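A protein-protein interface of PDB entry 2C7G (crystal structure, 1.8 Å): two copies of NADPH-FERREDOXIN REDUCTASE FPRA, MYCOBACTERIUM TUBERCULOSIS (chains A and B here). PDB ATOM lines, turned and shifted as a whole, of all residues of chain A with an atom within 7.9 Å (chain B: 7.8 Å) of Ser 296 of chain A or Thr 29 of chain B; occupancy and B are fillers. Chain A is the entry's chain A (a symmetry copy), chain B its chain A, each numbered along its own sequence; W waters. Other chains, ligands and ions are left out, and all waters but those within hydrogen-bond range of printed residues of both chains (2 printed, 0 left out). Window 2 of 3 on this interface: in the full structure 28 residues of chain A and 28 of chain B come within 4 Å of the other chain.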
ATOM      1  N   GLU A 293       3.574  10.110  14.677  1.00  0.00           N
ATOM      2  CA  GLU A 293       4.566  11.039  14.148  1.00  0.00           C
ATOM      3  C   GLU A 293       3.912  11.786  12.973  1.00  0.00           C
ATOM      4  O   GLU A 293       2.990  11.271  12.338  1.00  0.00           O
ATOM      5  CB  GLU A 293       5.835  10.295  13.725  1.00  0.00           C
ATOM      6  CG  GLU A 293       5.613   9.221  12.670  1.00  0.00           C
ATOM      7  CD  GLU A 293       6.807   8.284  12.473  1.00  0.00           C
ATOM      8  OE1 GLU A 293       7.834   8.425  13.187  1.00  0.00           O
ATOM      9  OE2 GLU A 293       6.695   7.387  11.608  1.00  0.00           O
ATOM     10  N   LEU A 294       4.371  13.007  12.697  1.00  0.00           N
ATOM     11  CA  LEU A 294       3.837  13.758  11.561  1.00  0.00           C
ATOM     12  C   LEU A 294       4.594  13.423  10.278  1.00  0.00           C
ATOM     13  O   LEU A 294       5.836  13.439  10.257  1.00  0.00           O
ATOM     14  CB  LEU A 294       3.860  15.269  11.830  1.00  0.00           C
ATOM     15  CG  LEU A 294       3.092  15.765  13.061  1.00  0.00           C
ATOM     16  CD1 LEU A 294       3.410  17.233  13.340  1.00  0.00           C
ATOM     17  CD2 LEU A 294       1.582  15.558  12.896  1.00  0.00           C
ATOM     18  N   VAL A 295       3.837  13.103   9.224  1.00  0.00           N
ATOM     19  CA  VAL A 295       4.408  12.692   7.936  1.00  0.00           C
ATOM     20  C   VAL A 295       3.627  13.355   6.800  1.00  0.00           C
ATOM     21  O   VAL A 295       2.387  13.457   6.859  1.00  0.00           O
ATOM     22  CB  VAL A 295       4.387  11.140   7.758  1.00  0.00           C
ATOM     23  CG1 VAL A 295       5.055  10.718   6.449  1.00  0.00           C
ATOM     24  CG2 VAL A 295       5.067  10.440   8.928  1.00  0.00           C
ATOM     25  N   SER A 296       4.347  13.811   5.774  1.00  0.00           N
ATOM     26  CA  SER A 296       3.702  14.357   4.579  1.00  0.00           C
ATOM     27  C   SER A 296       3.066  13.222   3.810  1.00  0.00           C
ATOM     28  O   SER A 296       3.688  12.168   3.622  1.00  0.00           O
ATOM     29  CB  SER A 296       4.717  15.066   3.685  1.00  0.00           C
ATOM     30  OG  SER A 296       5.262  16.184   4.349  1.00  0.00           O
ATOM     31  N   ASP A 297       1.827  13.412   3.366  1.00  0.00           N
ATOM     32  CA  ASP A 297       1.216  12.389   2.512  1.00  0.00           C
ATOM     33  C   ASP A 297       1.068  12.874   1.070  1.00  0.00           C
ATOM     34  O   ASP A 297       0.447  12.203   0.248  1.00  0.00           O
ATOM     35  CB  ASP A 297      -0.114  11.889   3.088  1.00  0.00           C
ATOM     36  CG  ASP A 297      -1.163  12.967   3.164  1.00  0.00           C
ATOM     37  OD1 ASP A 297      -0.913  14.096   2.691  1.00  0.00           O
ATOM     38  OD2 ASP A 297      -2.242  12.680   3.713  1.00  0.00           O
ATOM     39  N   GLY A 298       1.626  14.054   0.794  1.00  0.00           N
ATOM     40  CA  GLY A 298       1.630  14.635  -0.556  1.00  0.00           C
ATOM     41  C   GLY A 298       0.467  15.568  -0.817  1.00  0.00           C
ATOM     42  O   GLY A 298       0.384  16.175  -1.883  1.00  0.00           O
ATOM     43  N   SER A 299      -0.440  15.676   0.154  1.00  0.00           N
ATOM     44  CA  SER A 299      -1.674  16.458  -0.007  1.00  0.00           C
ATOM     45  C   SER A 299      -1.509  17.916   0.394  1.00  0.00           C
ATOM     46  O   SER A 299      -2.437  18.714   0.224  1.00  0.00           O
ATOM     47  CB  SER A 299      -2.794  15.863   0.837  1.00  0.00           C
ATOM     48  OG  SER A 299      -2.576  16.190   2.201  1.00  0.00           O
ATOM     49  N   GLY A 300      -0.349  18.266   0.944  1.00  0.00           N
ATOM     50  CA  GLY A 300      -0.141  19.615   1.470  1.00  0.00           C
ATOM     51  C   GLY A 300      -0.572  19.720   2.927  1.00  0.00           C
ATOM     52  O   GLY A 300      -0.461  20.776   3.543  1.00  0.00           O
ATOM     53  N   ARG A 301      -1.085  18.622   3.470  1.00  0.00           N
ATOM     54  CA  ARG A 301      -1.284  18.493   4.899  1.00  0.00           C
ATOM     55  C   ARG A 301      -0.125  17.676   5.462  1.00  0.00           C
ATOM     56  O   ARG A 301       0.613  16.982   4.706  1.00  0.00           O
ATOM     57  CB  ARG A 301      -2.529  17.691   5.185  1.00  0.00           C
ATOM     58  CG  ARG A 301      -2.191  16.204   5.177  1.00  0.00           C
ATOM     59  CD  ARG A 301      -3.074  15.374   6.100  1.00  0.00           C
ATOM     60  NE  ARG A 301      -3.060  13.969   5.697  1.00  0.00           N
ATOM     61  CZ  ARG A 301      -3.715  12.970   6.298  1.00  0.00           C
ATOM     62  NH1 ARG A 301      -4.463  13.173   7.381  1.00  0.00           N
ATOM     63  NH2 ARG A 301      -3.599  11.742   5.801  1.00  0.00           N
ATOM     64  N   VAL A 302       0.033  17.728   6.778  1.00  0.00           N
ATOM     65  CA  VAL A 302       0.744  16.667   7.463  1.00  0.00           C
ATOM     66  C   VAL A 302      -0.319  15.724   8.000  1.00  0.00           C
ATOM     67  O   VAL A 302      -1.390  16.160   8.436  1.00  0.00           O
ATOM     68  CB  VAL A 302       1.607  17.151   8.641  1.00  0.00           C
ATOM     69  CG1 VAL A 302       2.999  17.490   8.176  1.00  0.00           C
ATOM     70  CG2 VAL A 302       0.936  18.310   9.368  1.00  0.00           C
ATOM     71  N   ALA A 303      -0.016  14.435   7.941  1.00  0.00           N
ATOM     72  CA  ALA A 303      -0.871  13.402   8.469  1.00  0.00           C
ATOM     73  C   ALA A 303      -0.242  12.883   9.753  1.00  0.00           C
ATOM     74  O   ALA A 303       0.979  12.910   9.895  1.00  0.00           O
ATOM     75  CB  ALA A 303      -0.966  12.271   7.469  1.00  0.00           C
ATOM     76  N   ALA A 304      -1.071  12.419  10.684  1.00  0.00           N
ATOM     77  CA  ALA A 304      -0.573  11.596  11.780  1.00  0.00           C
ATOM     78  C   ALA A 304      -0.411  10.148  11.300  1.00  0.00           C
ATOM     79  O   ALA A 304      -1.305   9.600  10.653  1.00  0.00           O
ATOM     80  CB  ALA A 304      -1.504  11.665  12.984  1.00  0.00           C
ATOM     81  N   LYS A 305       0.742   9.556  11.604  1.00  0.00           N
ATOM     82  CA  LYS A 305       1.019   8.135  11.340  1.00  0.00           C
ATOM     83  C   LYS A 305       1.340   7.421  12.652  1.00  0.00           C
ATOM     84  O   LYS A 305       2.182   7.873  13.423  1.00  0.00           O
ATOM     85  CB  LYS A 305       2.200   8.006  10.373  1.00  0.00           C
ATOM     86  CG  LYS A 305       2.565   6.587   9.985  1.00  0.00           C
ATOM     87  CD  LYS A 305       3.684   6.576   8.943  1.00  0.00           C
ATOM     88  CE  LYS A 305       3.810   5.206   8.300  1.00  0.00           C
ATOM     89  NZ  LYS A 305       4.460   5.309   6.969  1.00  0.00           N
ATOM     90  N   LEU B  22      -0.481  15.801  -9.706  1.00  0.00           N
ATOM     91  CA  LEU B  22      -0.229  14.432  -9.236  1.00  0.00           C
ATOM     92  C   LEU B  22       1.252  14.035  -9.285  1.00  0.00           C
ATOM     93  O   LEU B  22       1.798  13.491  -8.319  1.00  0.00           O
ATOM     94  CB  LEU B  22      -1.051  13.437 -10.055  1.00  0.00           C
ATOM     95  CG  LEU B  22      -2.560  13.509  -9.838  1.00  0.00           C
ATOM     96  CD1 LEU B  22      -3.281  12.892 -11.033  1.00  0.00           C
ATOM     97  CD2 LEU B  22      -2.938  12.843  -8.527  1.00  0.00           C
ATOM     98  N   LEU B  23       1.898  14.310 -10.413  1.00  0.00           N
ATOM     99  CA  LEU B  23       3.302  13.947 -10.579  1.00  0.00           C
ATOM    100  C   LEU B  23       4.221  14.772  -9.671  1.00  0.00           C
ATOM    101  O   LEU B  23       5.210  14.245  -9.158  1.00  0.00           O
ATOM    102  CB  LEU B  23       3.720  14.017 -12.059  1.00  0.00           C
ATOM    103  CG  LEU B  23       2.924  13.096 -13.002  1.00  0.00           C
ATOM    104  CD1 LEU B  23       3.153  13.458 -14.469  1.00  0.00           C
ATOM    105  CD2 LEU B  23       3.231  11.599 -12.758  1.00  0.00           C
ATOM    106  N   LYS B  24       3.884  16.044  -9.451  1.00  0.00           N
ATOM    107  CA  LYS B  24       4.679  16.928  -8.570  1.00  0.00           C
ATOM    108  C   LYS B  24       4.593  16.456  -7.109  1.00  0.00           C
ATOM    109  O   LYS B  24       5.577  16.511  -6.367  1.00  0.00           O
ATOM    110  CB  LYS B  24       4.231  18.385  -8.694  1.00  0.00           C
ATOM    111  CG  LYS B  24       5.076  19.392  -7.888  1.00  0.00           C
ATOM    112  N   ALA B  25       3.413  15.998  -6.703  1.00  0.00           N
ATOM    113  CA  ALA B  25       3.225  15.407  -5.381  1.00  0.00           C
ATOM    114  C   ALA B  25       4.114  14.171  -5.196  1.00  0.00           C
ATOM    115  O   ALA B  25       4.752  14.011  -4.155  1.00  0.00           O
ATOM    116  CB  ALA B  25       1.758  15.049  -5.162  1.00  0.00           C
ATOM    117  N   ALA B  26       4.149  13.297  -6.198  1.00  0.00           N
ATOM    118  CA  ALA B  26       5.040  12.135  -6.166  1.00  0.00           C
ATOM    119  C   ALA B  26       6.501  12.592  -6.082  1.00  0.00           C
ATOM    120  O   ALA B  26       7.269  12.074  -5.269  1.00  0.00           O
ATOM    121  CB  ALA B  26       4.816  11.236  -7.394  1.00  0.00           C
ATOM    122  N   ASP B  27       6.863  13.570  -6.911  1.00  0.00           N
ATOM    123  CA  ASP B  27       8.234  14.085  -6.988  1.00  0.00           C
ATOM    124  C   ASP B  27       8.738  14.736  -5.691  1.00  0.00           C
ATOM    125  O   ASP B  27       9.951  14.813  -5.464  1.00  0.00           O
ATOM    126  CB  ASP B  27       8.352  15.122  -8.107  1.00  0.00           C
ATOM    127  CG  ASP B  27       8.288  14.517  -9.502  1.00  0.00           C
ATOM    128  OD1 ASP B  27       8.276  13.283  -9.650  1.00  0.00           O
ATOM    129  OD2 ASP B  27       8.252  15.308 -10.460  1.00  0.00           O
ATOM    130  N   THR B  28       7.819  15.231  -4.866  1.00  0.00           N
ATOM    131  CA  THR B  28       8.201  15.980  -3.664  1.00  0.00           C
ATOM    132  C   THR B  28       7.868  15.227  -2.369  1.00  0.00           C
ATOM    133  O   THR B  28       8.058  15.767  -1.264  1.00  0.00           O
ATOM    134  CB  THR B  28       7.546  17.401  -3.625  1.00  0.00           C
ATOM    135  OG1 THR B  28       6.118  17.286  -3.631  1.00  0.00           O
ATOM    136  CG2 THR B  28       7.986  18.258  -4.799  1.00  0.00           C
ATOM    137  N   THR B  29       7.381  13.998  -2.502  1.00  0.00           N
ATOM    138  CA  THR B  29       6.913  13.202  -1.357  1.00  0.00           C
ATOM    139  C   THR B  29       7.533  11.804  -1.279  1.00  0.00           C
ATOM    140  O   THR B  29       7.390  10.990  -2.191  1.00  0.00           O
ATOM    141  CB  THR B  29       5.361  13.091  -1.335  1.00  0.00           C
ATOM    142  OG1 THR B  29       4.790  14.391  -1.530  1.00  0.00           O
ATOM    143  CG2 THR B  29       4.866  12.506  -0.016  1.00  0.00           C
ATOM    144  N   GLU B  30       8.201  11.529  -0.158  1.00  0.00           N
ATOM    145  CA  GLU B  30       8.720  10.198   0.137  1.00  0.00           C
ATOM    146  C   GLU B  30       7.584   9.188   0.234  1.00  0.00           C
ATOM    147  O   GLU B  30       6.505   9.509   0.745  1.00  0.00           O
ATOM    148  CB  GLU B  30       9.502  10.212   1.455  1.00  0.00           C
ATOM    149  N   ASP B  31       7.840   7.980  -0.273  1.00  0.00           N
ATOM    150  CA  ASP B  31       6.890   6.865  -0.260  1.00  0.00           C
ATOM    151  C   ASP B  31       5.567   7.190  -0.944  1.00  0.00           C
ATOM    152  O   ASP B  31       4.494   6.785  -0.476  1.00  0.00           O
ATOM    153  CB  ASP B  31       6.654   6.372   1.174  1.00  0.00           C
ATOM    154  CG  ASP B  31       7.926   5.917   1.846  1.00  0.00           C
ATOM    155  OD1 ASP B  31       8.592   5.003   1.312  1.00  0.00           O
ATOM    156  OD2 ASP B  31       8.260   6.476   2.908  1.00  0.00           O
ATOM    157  N   LEU B  32       5.650   7.942  -2.039  1.00  0.00           N
ATOM    158  CA  LEU B  32       4.478   8.294  -2.834  1.00  0.00           C
ATOM    159  C   LEU B  32       4.888   8.291  -4.292  1.00  0.00           C
ATOM    160  O   LEU B  32       5.742   9.067  -4.699  1.00  0.00           O
ATOM    161  CB  LEU B  32       3.918   9.674  -2.453  1.00  0.00           C
ATOM    162  CG  LEU B  32       2.645  10.117  -3.201  1.00  0.00           C
ATOM    163  CD1 LEU B  32       1.453   9.222  -2.855  1.00  0.00           C
ATOM    164  CD2 LEU B  32       2.313  11.581  -2.916  1.00  0.00           C
ATOM    165  N   ASP B  33       4.271   7.405  -5.063  1.00  0.00           N
ATOM    166  CA  ASP B  33       4.565   7.293  -6.478  1.00  0.00           C
ATOM    167  C   ASP B  33       3.268   7.265  -7.269  1.00  0.00           C
ATOM    168  O   ASP B  33       2.240   6.802  -6.781  1.00  0.00           O
ATOM    169  CB  ASP B  33       5.429   6.060  -6.751  1.00  0.00           C
ATOM    170  CG  ASP B  33       6.841   6.205  -6.176  1.00  0.00           C
ATOM    171  OD1 ASP B  33       7.626   7.013  -6.711  1.00  0.00           O
ATOM    172  OD2 ASP B  33       7.163   5.517  -5.182  1.00  0.00           O
ATOM    173  N   ILE B 383      -5.362  12.963  -3.009  1.00  0.00           N
ATOM    174  CA  ILE B 383      -4.177  12.392  -2.372  1.00  0.00           C
ATOM    175  C   ILE B 383      -4.369  12.206  -0.854  1.00  0.00           C
ATOM    176  O   ILE B 383      -3.952  11.186  -0.284  1.00  0.00           O
ATOM    177  CB  ILE B 383      -2.916  13.252  -2.709  1.00  0.00           C
ATOM    178  CG1 ILE B 383      -2.646  13.192  -4.230  1.00  0.00           C
ATOM    179  CG2 ILE B 383      -1.702  12.825  -1.874  1.00  0.00           C
ATOM    180  CD1 ILE B 383      -1.545  14.145  -4.715  1.00  0.00           C
ATOM    181  N   LYS B 390      -4.630   4.391   3.044  1.00  0.00           N
ATOM    182  CA  LYS B 390      -3.370   3.692   3.278  1.00  0.00           C
ATOM    183  C   LYS B 390      -3.076   3.505   4.775  1.00  0.00           C
ATOM    184  O   LYS B 390      -2.787   2.385   5.211  1.00  0.00           O
ATOM    185  CB  LYS B 390      -2.216   4.422   2.585  1.00  0.00           C
ATOM    186  CG  LYS B 390      -0.904   3.646   2.532  1.00  0.00           C
ATOM    187  CD  LYS B 390       0.268   4.595   2.288  1.00  0.00           C
ATOM    188  CE  LYS B 390       1.590   3.853   2.146  1.00  0.00           C
ATOM    189  NZ  LYS B 390       2.725   4.812   2.003  1.00  0.00           N
HETATM  190  O   HOH W   1      -1.474  10.120   0.068  1.00  0.00           O
HETATM  191  O   HOH W   2       6.054  10.787   3.171  1.00  0.00           O
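Water W1 lies within hydrogen-bond range of O of Ile 383 of chain B (2.7 Å) and O of Asp 297 of chain A (2.8 Å). Water W2 bridges the backbone carbonyl oxygen (O) of Ser 296 of chain A (2.8 Å) and the backbone carbonyl oxygen (O) of Glu 30 of chain B (2.8 Å).
Printed residues of chain A that touch a printed residue of chain B: Ser 296, Asp 297, Gly 298 and Ser 299. Among the printed residues, no Asp or Glu carboxylate lies within 4 Å of a Lys or Arg side-chain nitrogen of the other chain.
No position is printed for both chains.
O of Ala 25 of chain B lies within hydrogen-bond range of OG1 of Thr 29 of chain B, at 2.7 Å. The side-chain carboxylate (OD1) of Asp 297 of chain A is in hydrogen-bond range of the side-chain hydroxyl (OG) of Ser 299 of chain A, at 2.7 Å. The guanidinium group (NE) of Arg 301 of chain A lies within salt-bridge range of the side-chain carboxylate (OD2) of Asp 297 of chain A (2.5 Å). N of Arg 301 of chain A lies close to OG of Ser 299 of chain A (3.1 Å).
Of chain B, only Thr 29 comes within 4 Å of Ser 296 of chain A. Of chain A, only Ser 296, Asp 297 and Gly 298 come within 4 Å of Thr 29 of chain B. Printed residues of chain B within 4 Å of Gly 298 of chain A: Ala 25, Thr 29, Leu 32 and Ile 383. Printed residues of chain B within 4 Å of Ser 299 of chain A: Ile 383. Printed residues of chain A within 4 Å of Ala 25 of chain B: Gly 298. Lys 24 of chain B touches none of the printed residues of chain A. Asp 27 of chain B touches none of the printed residues of chain A. The nearest printed residue of chain B that does not touch Ser 299 of chain A is Thr 29 of chain B (5.6 Å).
Ser 296 of chain A touches Thr 29 of chain B. Asp 297 of chain A touches Thr 29 of chain B. CD2 of Leu 32 of chain B touches O of Asp 297 of chain A, 3.7 Å away. Asp 297 of chain A touches Ile 383 of chain B. O of Gly 298 of chain A touches CB of Ala 25 of chain B, at 3.7 Å. Thr 29 of chain B touches Gly 298 of chain A (OG1 to CA, 3.3 Å). Leu 32 of chain B touches Gly 298 of chain A. Gly 298 of chain A touches Ile 383 of chain B (C to CG2, 3.7 Å). N of Ser 299 of chain A touches CG2 of Ile 383 of chain B, 3.7 Å away.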
